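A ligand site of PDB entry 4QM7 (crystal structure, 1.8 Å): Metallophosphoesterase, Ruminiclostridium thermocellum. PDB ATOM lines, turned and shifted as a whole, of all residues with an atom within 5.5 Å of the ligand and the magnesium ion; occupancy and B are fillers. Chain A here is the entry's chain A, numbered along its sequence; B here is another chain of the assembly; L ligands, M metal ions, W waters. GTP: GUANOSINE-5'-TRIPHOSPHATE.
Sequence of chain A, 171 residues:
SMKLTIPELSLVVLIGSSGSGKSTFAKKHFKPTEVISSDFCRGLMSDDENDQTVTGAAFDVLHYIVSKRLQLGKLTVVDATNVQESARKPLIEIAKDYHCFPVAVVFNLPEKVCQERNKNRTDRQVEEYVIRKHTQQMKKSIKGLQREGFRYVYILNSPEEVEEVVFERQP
The magnesium ion is bound by water W7, water W9, the side-chain hydroxyl of Ser 23, an oxygen (O3G) of the ligand, an oxygen (O1B) of the ligand and water W2. The magnesium ion has six donor atoms within binding distance.
Water W10 lies within hydrogen-bond range of OP1 of DC 1 of chain B (2.5 Å), O1G of the ligand (2.5 Å), NH1 of Arg 124 (3.0 Å) and NH1 of Arg 121 (3.4 Å). Water W1 bridges an oxygen (O1A) of the ligand and the side-chain carboxylate of Asp 123. Water W11 lies within hydrogen-bond range of O of Arg 117 (2.8 Å), O3' of the ligand (2.8 Å) and N of Arg 121 (3.4 Å). Water W6 bridges O of Gly 21 and N7 of the ligand. Water W3 lies within hydrogen-bond range of OG1 of Thr 24 (2.7 Å) and O2' of the ligand (3.3 Å). Water W13 lies within hydrogen-bond range of NH2 of Arg 117 (2.7 Å) and O6 of the ligand (3.4 Å).
O of Ser 17 touches O2B of the ligand, 3.7 Å away. Arg 117 touches the ligand. DC 1 of chain B touches the ligand (C5' to O1G, 3.6 Å).
One residue has an atom within 4 Å of the magnesium ion: Ser 23.
The backbone NH of Ser 23 is in hydrogen-bond range of an oxygen (O2A) of the ligand, 3.4 Å away. O2A of the ligand lies within hydrogen-bond range of N of Thr 24 (2.9 Å). The side-chain hydroxyl (OG1) of Thr 24 is in hydrogen-bond range of an oxygen (O2A) of the ligand, 2.6 Å away. O1G of the ligand is in hydrogen-bond range of OG of Ser 18, 2.6 Å away. An oxygen (O2B) of the ligand lies within hydrogen-bond range of the backbone NH (N) of Lys 22 (2.9 Å). NZ of Lys 22 lies within salt-bridge range of O2B of the ligand (2.8 Å). O1G of the ligand lies within salt-bridge range of NH1 of Arg 121, 3.0 Å away. The backbone NH (N) of Gly 21 lies within hydrogen-bond range of an oxygen (O2B) of the ligand, at 3.0 Å. NH1 of Arg 124 lies within salt-bridge range of O1G of the ligand. An oxygen (O3B) of the ligand lies within hydrogen-bond range of the backbone NH of Gly 19, at 3.1 Å. O2B of the ligand is in hydrogen-bond range of N of Ser 20 (3.4 Å).
The side-chain hydroxyl (OG) of Ser 23 lies close to the side-chain carboxylate (OD2) of Asp 79 (2.6 Å). The backbone carbonyl oxygen (O) of Ser 17 sits at hydrogen-bond distance from the side-chain amino group (NZ) of Lys 22, at 3.0 Å. The side-chain amino group (NZ) of Lys 22 sits at hydrogen-bond distance from the backbone carbonyl oxygen (O) of Gly 16. The backbone carbonyl oxygen (O) of Arg 124 lies within hydrogen-bond range of the guanidinium group (NE) of Arg 121, 3.1 Å away. The side-chain carboxylate (OD1) of Asp 123 is in salt-bridge range of the guanidinium group (NE) of Arg 121, at 2.9 Å. OP2 of DC 1 of chain B lies within salt-bridge range of the guanidinium group (NH1) of Arg 124 (2.8 Å). The backbone carbonyl oxygen (O) of Ser 20 sits at hydrogen-bond distance from the guanidinium group (NH1) of Arg 117 (3.1 Å). The side-chain hydroxyl of Ser 20 lies within hydrogen-bond range of the backbone carbonyl oxygen of Ser 17.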
ATOM      1  N   GLY A  16     -16.840  -9.231  11.232  1.00  0.00           N
ATOM      2  CA  GLY A  16     -16.130  -8.241  11.988  1.00  0.00           C
ATOM      3  C   GLY A  16     -17.040  -7.254  12.646  1.00  0.00           C
ATOM      4  O   GLY A  16     -18.079  -6.893  12.075  1.00  0.00           O
ATOM      5  N   SER A  17     -16.578  -6.738  13.775  1.00  0.00           N
ATOM      6  CA  SER A  17     -17.320  -5.677  14.503  1.00  0.00           C
ATOM      7  C   SER A  17     -17.533  -4.433  13.624  1.00  0.00           C
ATOM      8  O   SER A  17     -16.771  -4.132  12.747  1.00  0.00           O
ATOM      9  CB  SER A  17     -16.478  -5.291  15.735  1.00  0.00           C
ATOM     10  OG  SER A  17     -17.088  -4.206  16.473  1.00  0.00           O
ATOM     11  N   SER A  18     -18.562  -3.619  13.937  1.00  0.00           N
ATOM     12  CA  SER A  18     -18.581  -2.300  13.346  1.00  0.00           C
ATOM     13  C   SER A  18     -17.247  -1.619  13.653  1.00  0.00           C
ATOM     14  O   SER A  18     -16.713  -1.767  14.784  1.00  0.00           O
ATOM     15  CB  SER A  18     -19.740  -1.506  14.004  1.00  0.00           C
ATOM     16  OG  SER A  18     -19.719  -0.160  13.527  1.00  0.00           O
ATOM     17  N   GLY A  19     -16.664  -0.917  12.680  1.00  0.00           N
ATOM     18  CA  GLY A  19     -15.396  -0.237  12.932  1.00  0.00           C
ATOM     19  C   GLY A  19     -14.158  -1.059  12.596  1.00  0.00           C
ATOM     20  O   GLY A  19     -13.041  -0.513  12.602  1.00  0.00           O
ATOM     21  N   SER A  20     -14.346  -2.336  12.257  1.00  0.00           N
ATOM     22  CA  SER A  20     -13.183  -3.212  11.993  1.00  0.00           C
ATOM     23  C   SER A  20     -12.551  -3.017  10.597  1.00  0.00           C
ATOM     24  O   SER A  20     -11.438  -3.510  10.356  1.00  0.00           O
ATOM     25  CB  SER A  20     -13.524  -4.697  12.223  1.00  0.00           C
ATOM     26  OG  SER A  20     -14.585  -5.111  11.333  1.00  0.00           O
ATOM     27  N   GLY A  21     -13.260  -2.328   9.706  1.00  0.00           N
ATOM     28  CA  GLY A  21     -12.751  -1.954   8.406  1.00  0.00           C
ATOM     29  C   GLY A  21     -13.219  -2.813   7.235  1.00  0.00           C
ATOM     30  O   GLY A  21     -12.535  -2.897   6.181  1.00  0.00           O
ATOM     31  N   LYS A  22     -14.353  -3.488   7.425  1.00  0.00           N
ATOM     32  CA  LYS A  22     -14.898  -4.386   6.419  1.00  0.00           C
ATOM     33  C   LYS A  22     -15.165  -3.685   5.097  1.00  0.00           C
ATOM     34  O   LYS A  22     -14.817  -4.219   4.031  1.00  0.00           O
ATOM     35  CB  LYS A  22     -16.217  -5.026   6.893  1.00  0.00           C
ATOM     36  CG  LYS A  22     -16.120  -5.894   8.166  1.00  0.00           C
ATOM     37  CD  LYS A  22     -17.448  -6.484   8.575  1.00  0.00           C
ATOM     38  CE  LYS A  22     -18.448  -5.353   8.915  1.00  0.00           C
ATOM     39  NZ  LYS A  22     -18.100  -4.583  10.139  1.00  0.00           N
ATOM     40  N   SER A  23     -15.862  -2.552   5.148  1.00  0.00           N
ATOM     41  CA  SER A  23     -16.250  -1.903   3.894  1.00  0.00           C
ATOM     42  C   SER A  23     -15.049  -1.329   3.147  1.00  0.00           C
ATOM     43  O   SER A  23     -14.978  -1.384   1.911  1.00  0.00           O
ATOM     44  CB  SER A  23     -17.322  -0.826   4.149  1.00  0.00           C
ATOM     45  OG  SER A  23     -18.430  -1.444   4.766  1.00  0.00           O
ATOM     46  N   THR A  24     -14.088  -0.830   3.905  1.00  0.00           N
ATOM     47  CA  THR A  24     -12.870  -0.270   3.362  1.00  0.00           C
ATOM     48  C   THR A  24     -12.096  -1.388   2.666  1.00  0.00           C
ATOM     49  O   THR A  24     -11.582  -1.203   1.553  1.00  0.00           O
ATOM     50  CB  THR A  24     -12.034   0.337   4.484  1.00  0.00           C
ATOM     51  OG1 THR A  24     -12.770   1.406   5.095  1.00  0.00           O
ATOM     52  CG2 THR A  24     -10.728   0.922   3.925  1.00  0.00           C
ATOM     53  N   PHE A  25     -12.033  -2.526   3.344  1.00  0.00           N
ATOM     54  CA  PHE A  25     -11.354  -3.734   2.796  1.00  0.00           C
ATOM     55  C   PHE A  25     -12.053  -4.218   1.539  1.00  0.00           C
ATOM     56  O   PHE A  25     -11.399  -4.532   0.539  1.00  0.00           O
ATOM     57  CB  PHE A  25     -11.387  -4.804   3.895  1.00  0.00           C
ATOM     58  CG  PHE A  25     -10.727  -6.109   3.528  1.00  0.00           C
ATOM     59  CD1 PHE A  25     -11.483  -7.105   2.939  1.00  0.00           C
ATOM     60  CD2 PHE A  25      -9.398  -6.346   3.867  1.00  0.00           C
ATOM     61  CE1 PHE A  25     -10.948  -8.329   2.658  1.00  0.00           C
ATOM     62  CE2 PHE A  25      -8.822  -7.600   3.581  1.00  0.00           C
ATOM     63  CZ  PHE A  25      -9.610  -8.592   2.985  1.00  0.00           C
ATOM     64  N   ASP A  79     -20.950  -7.805   2.853  1.00  0.00           N
ATOM     65  CA  ASP A  79     -20.428  -6.759   3.718  1.00  0.00           C
ATOM     66  C   ASP A  79     -21.443  -6.398   4.838  1.00  0.00           C
ATOM     67  O   ASP A  79     -22.266  -5.520   4.694  1.00  0.00           O
ATOM     68  CB  ASP A  79     -19.999  -5.539   2.880  1.00  0.00           C
ATOM     69  CG  ASP A  79     -19.442  -4.419   3.726  1.00  0.00           C
ATOM     70  OD1 ASP A  79     -19.090  -4.665   4.891  1.00  0.00           O
ATOM     71  OD2 ASP A  79     -19.332  -3.280   3.206  1.00  0.00           O
ATOM     72  N   THR A  81     -21.790  -7.331   9.520  1.00  0.00           N
ATOM     73  CA  THR A  81     -20.939  -7.770  10.639  1.00  0.00           C
ATOM     74  C   THR A  81     -20.790  -9.281  10.659  1.00  0.00           C
ATOM     75  O   THR A  81     -19.648  -9.800  10.893  1.00  0.00           O
ATOM     76  CB  THR A  81     -21.435  -7.275  11.995  1.00  0.00           C
ATOM     77  OG1 THR A  81     -22.790  -7.714  12.194  1.00  0.00           O
ATOM     78  CG2 THR A  81     -21.321  -5.744  12.063  1.00  0.00           C
ATOM     79  N   ARG A 117     -11.438   3.601  15.855  1.00  0.00           N
ATOM     80  CA  ARG A 117     -11.853   3.921  14.490  1.00  0.00           C
ATOM     81  C   ARG A 117     -13.267   4.436  14.462  1.00  0.00           C
ATOM     82  O   ARG A 117     -13.605   5.299  13.659  1.00  0.00           O
ATOM     83  CB  ARG A 117     -11.750   2.694  13.585  1.00  0.00           C
ATOM     84  CG  ARG A 117     -10.310   2.266  13.423  1.00  0.00           C
ATOM     85  CD  ARG A 117     -10.256   1.096  12.534  1.00  0.00           C
ATOM     86  NE  ARG A 117      -8.880   0.730  12.221  1.00  0.00           N
ATOM     87  CZ  ARG A 117      -8.581  -0.325  11.470  1.00  0.00           C
ATOM     88  NH1 ARG A 117      -9.569  -1.085  11.015  1.00  0.00           N
ATOM     89  NH2 ARG A 117      -7.316  -0.633  11.217  1.00  0.00           N
ATOM     90  N   ASN A 120     -13.372   8.100  15.475  1.00  0.00           N
ATOM     91  CA  ASN A 120     -12.768   9.010  14.515  1.00  0.00           C
ATOM     92  C   ASN A 120     -13.433   9.038  13.138  1.00  0.00           C
ATOM     93  O   ASN A 120     -13.024   9.819  12.260  1.00  0.00           O
ATOM     94  CB  ASN A 120     -11.273   8.668  14.336  1.00  0.00           C
ATOM     95  CG  ASN A 120     -10.461   9.041  15.558  1.00  0.00           C
ATOM     96  OD1 ASN A 120     -10.700  10.077  16.184  1.00  0.00           O
ATOM     97  ND2 ASN A 120      -9.479   8.188  15.907  1.00  0.00           N
ATOM     98  N   ARG A 121     -14.437   8.200  12.923  1.00  0.00           N
ATOM     99  CA  ARG A 121     -15.045   8.176  11.594  1.00  0.00           C
ATOM    100  C   ARG A 121     -16.013   9.337  11.468  1.00  0.00           C
ATOM    101  O   ARG A 121     -16.624   9.777  12.458  1.00  0.00           O
ATOM    102  CB  ARG A 121     -15.716   6.824  11.253  1.00  0.00           C
ATOM    103  CG  ARG A 121     -16.859   6.427  12.165  1.00  0.00           C
ATOM    104  CD  ARG A 121     -17.218   4.949  11.926  1.00  0.00           C
ATOM    105  NE  ARG A 121     -17.852   4.715  10.620  1.00  0.00           N
ATOM    106  CZ  ARG A 121     -18.273   3.526  10.205  1.00  0.00           C
ATOM    107  NH1 ARG A 121     -18.119   2.457  10.991  1.00  0.00           N
ATOM    108  NH2 ARG A 121     -18.856   3.395   9.020  1.00  0.00           N
ATOM    109  N   THR A 122     -16.119   9.838  10.243  1.00  0.00           N
ATOM    110  CA  THR A 122     -16.922  11.031   9.973  1.00  0.00           C
ATOM    111  C   THR A 122     -18.222  10.699   9.267  1.00  0.00           C
ATOM    112  O   THR A 122     -19.025  11.598   9.043  1.00  0.00           O
ATOM    113  CB  THR A 122     -16.157  12.019   9.059  1.00  0.00           C
ATOM    114  OG1 THR A 122     -15.692  11.331   7.887  1.00  0.00           O
ATOM    115  CG2 THR A 122     -14.954  12.621   9.816  1.00  0.00           C
ATOM    116  N   ASP A 123     -18.407   9.426   8.914  1.00  0.00           N
ATOM    117  CA  ASP A 123     -19.605   9.001   8.143  1.00  0.00           C
ATOM    118  C   ASP A 123     -20.846   8.602   8.961  1.00  0.00           C
ATOM    119  O   ASP A 123     -21.924   9.166   8.717  1.00  0.00           O
ATOM    120  CB  ASP A 123     -19.273   7.941   7.053  1.00  0.00           C
ATOM    121  CG  ASP A 123     -18.625   6.639   7.602  1.00  0.00           C
ATOM    122  OD1 ASP A 123     -17.798   6.702   8.539  1.00  0.00           O
ATOM    123  OD2 ASP A 123     -18.930   5.554   7.039  1.00  0.00           O
ATOM    124  N   ARG A 124     -20.719   7.626   9.877  1.00  0.00           N
ATOM    125  CA  ARG A 124     -21.829   7.099  10.719  1.00  0.00           C
ATOM    126  C   ARG A 124     -21.293   6.172  11.851  1.00  0.00           C
ATOM    127  O   ARG A 124     -20.771   5.071  11.628  1.00  0.00           O
ATOM    128  CB  ARG A 124     -22.940   6.394   9.938  1.00  0.00           C
ATOM    129  CG  ARG A 124     -22.460   5.250   9.084  1.00  0.00           C
ATOM    130  CD  ARG A 124     -23.523   4.177   8.719  1.00  0.00           C
ATOM    131  NE  ARG A 124     -23.159   3.522   7.461  1.00  0.00           N
ATOM    132  CZ  ARG A 124     -22.613   2.294   7.279  1.00  0.00           C
ATOM    133  NH1 ARG A 124     -22.386   1.434   8.258  1.00  0.00           N
ATOM    134  NH2 ARG A 124     -22.328   1.917   6.041  1.00  0.00           N
ATOM    135  N   VAL A 126     -21.435   4.195  15.739  1.00  0.00           N
ATOM    136  CA  VAL A 126     -22.316   3.432  16.604  1.00  0.00           C
ATOM    137  C   VAL A 126     -21.935   3.720  18.053  1.00  0.00           C
ATOM    138  O   VAL A 126     -20.880   4.310  18.340  1.00  0.00           O
ATOM    139  CB  VAL A 126     -22.228   1.910  16.350  1.00  0.00           C
ATOM    140  CG1 VAL A 126     -22.721   1.527  14.953  1.00  0.00           C
ATOM    141  CG2 VAL A 126     -20.809   1.378  16.562  1.00  0.00           C
ATOM    142  N   VAL A 162      -4.213  -7.307   8.093  1.00  0.00           N
ATOM    143  CA  VAL A 162      -5.241  -6.857   7.157  1.00  0.00           C
ATOM    144  C   VAL A 162      -4.648  -6.120   5.954  1.00  0.00           C
ATOM    145  O   VAL A 162      -5.030  -6.397   4.801  1.00  0.00           O
ATOM    146  CB  VAL A 162      -6.278  -5.918   7.837  1.00  0.00           C
ATOM    147  CG1 VAL A 162      -7.264  -5.419   6.782  1.00  0.00           C
ATOM    148  CG2 VAL A 162      -7.007  -6.684   8.922  1.00  0.00           C
ATOM    149  OP3  DC B   1     -26.206   1.387  11.329  1.00  0.00           O
ATOM    150  P    DC B   1     -24.811   1.063  10.970  1.00  0.00           P
ATOM    151  OP1  DC B   1     -23.977   2.240  11.317  1.00  0.00           O
ATOM    152  OP2  DC B   1     -24.700   0.480   9.613  1.00  0.00           O
ATOM    153  O5'  DC B   1     -24.508  -0.175  11.919  1.00  0.00           O
ATOM    154  C5'  DC B   1     -23.273  -0.877  11.763  1.00  0.00           C
ATOM    155  C4'  DC B   1     -23.473  -2.311  12.200  1.00  0.00           C
ATOM    156  O4'  DC B   1     -23.735  -2.283  13.628  1.00  0.00           O
ATOM    157  C3'  DC B   1     -24.684  -3.019  11.573  1.00  0.00           C
ATOM    158  O3'  DC B   1     -24.406  -4.424  11.443  1.00  0.00           O
ATOM    159  C2'  DC B   1     -25.783  -2.842  12.625  1.00  0.00           C
ATOM    160  C1'  DC B   1     -24.964  -2.926  13.899  1.00  0.00           C
ATOM    161  N1   DC B   1     -25.621  -2.267  15.052  1.00  0.00           N
ATOM    162  C2   DC B   1     -25.947  -3.066  16.157  1.00  0.00           C
ATOM    163  O2   DC B   1     -25.681  -4.260  16.145  1.00  0.00           O
ATOM    164  N3   DC B   1     -26.601  -2.479  17.187  1.00  0.00           N
ATOM    165  C4   DC B   1     -26.857  -1.180  17.161  1.00  0.00           C
ATOM    166  N4   DC B   1     -27.509  -0.643  18.224  1.00  0.00           N
ATOM    167  C5   DC B   1     -26.507  -0.364  16.044  1.00  0.00           C
ATOM    168  C6   DC B   1     -25.896  -0.945  14.996  1.00  0.00           C
HETATM  169  PG  GTP L   1     -19.524  -0.925   9.830  1.00  0.00           P
HETATM  170  O1G GTP L   1     -19.961   0.074  10.899  1.00  0.00           O
HETATM  171  O2G GTP L   1     -19.832  -2.361  10.277  1.00  0.00           O
HETATM  172  O3G GTP L   1     -20.102  -0.641   8.465  1.00  0.00           O
HETATM  173  O3B GTP L   1     -17.905  -0.673   9.847  1.00  0.00           O
HETATM  174  PB  GTP L   1     -16.816  -1.293   8.855  1.00  0.00           P
HETATM  175  O1B GTP L   1     -17.409  -1.398   7.471  1.00  0.00           O
HETATM  176  O2B GTP L   1     -16.283  -2.566   9.433  1.00  0.00           O
HETATM  177  O3A GTP L   1     -15.678  -0.213   8.880  1.00  0.00           O
HETATM  178  PA  GTP L   1     -15.255   0.857   7.777  1.00  0.00           P
HETATM  179  O1A GTP L   1     -16.372   1.792   7.504  1.00  0.00           O
HETATM  180  O2A GTP L   1     -14.590   0.224   6.588  1.00  0.00           O
HETATM  181  O5' GTP L   1     -14.052   1.632   8.532  1.00  0.00           O
HETATM  182  C5' GTP L   1     -14.430   2.446   9.631  1.00  0.00           C
HETATM  183  C4' GTP L   1     -13.384   3.547   9.863  1.00  0.00           C
HETATM  184  O4' GTP L   1     -12.127   2.912  10.008  1.00  0.00           O
HETATM  185  C3' GTP L   1     -13.314   4.511   8.695  1.00  0.00           C
HETATM  186  O3' GTP L   1     -13.160   5.821   9.214  1.00  0.00           O
HETATM  187  C2' GTP L   1     -12.070   4.039   7.997  1.00  0.00           C
HETATM  188  O2' GTP L   1     -11.418   5.088   7.287  1.00  0.00           O
HETATM  189  C1' GTP L   1     -11.191   3.452   9.101  1.00  0.00           C
HETATM  190  N9  GTP L   1     -10.396   2.339   8.577  1.00  0.00           N
HETATM  191  C8  GTP L   1     -10.904   1.239   7.936  1.00  0.00           C
HETATM  192  N7  GTP L   1      -9.881   0.425   7.569  1.00  0.00           N
HETATM  193  C5  GTP L   1      -8.727   1.004   7.976  1.00  0.00           C
HETATM  194  C6  GTP L   1      -7.403   0.609   7.875  1.00  0.00           C
HETATM  195  O6  GTP L   1      -7.144  -0.461   7.305  1.00  0.00           O
HETATM  196  N1  GTP L   1      -6.409   1.407   8.401  1.00  0.00           N
HETATM  197  C2  GTP L   1      -6.756   2.593   9.022  1.00  0.00           C
HETATM  198  N2  GTP L   1      -5.792   3.378   9.537  1.00  0.00           N
HETATM  199  N3  GTP L   1      -8.058   2.985   9.121  1.00  0.00           N
HETATM  200  C4  GTP L   1      -9.035   2.198   8.609  1.00  0.00           C
HETATM  201 MG    MG M   1     -19.285  -1.010   6.593  1.00  0.00          MG
HETATM  202  O   HOH W   1     -16.309   4.256   6.462  1.00  0.00           O
HETATM  203  O   HOH W   2     -18.698   1.007   6.364  1.00  0.00           O
HETATM  204  O   HOH W   3     -12.202   3.943   4.285  1.00  0.00           O
HETATM  205  O   HOH W   4     -14.251   8.114   8.146  1.00  0.00           O
HETATM  206  O   HOH W   5     -10.032   7.273   8.098  1.00  0.00           O
HETATM  207  O   HOH W   6      -9.745  -2.288   6.359  1.00  0.00           O
HETATM  208  O   HOH W   7     -19.805  -2.933   6.621  1.00  0.00           O
HETATM  209  O   HOH W   8     -21.570  -3.791   8.714  1.00  0.00           O
HETATM  210  O   HOH W   9     -21.037  -0.565   5.655  1.00  0.00           O
HETATM  211  O   HOH W  10     -21.487   2.105  11.088  1.00  0.00           O
HETATM  212  O   HOH W  11     -11.871   6.263  11.690  1.00  0.00           O
HETATM  213  O   HOH W  12      -4.891  -2.077   8.267  1.00  0.00           O
HETATM  214  O   HOH W  13      -6.833  -2.847   9.749  1.00  0.00           O
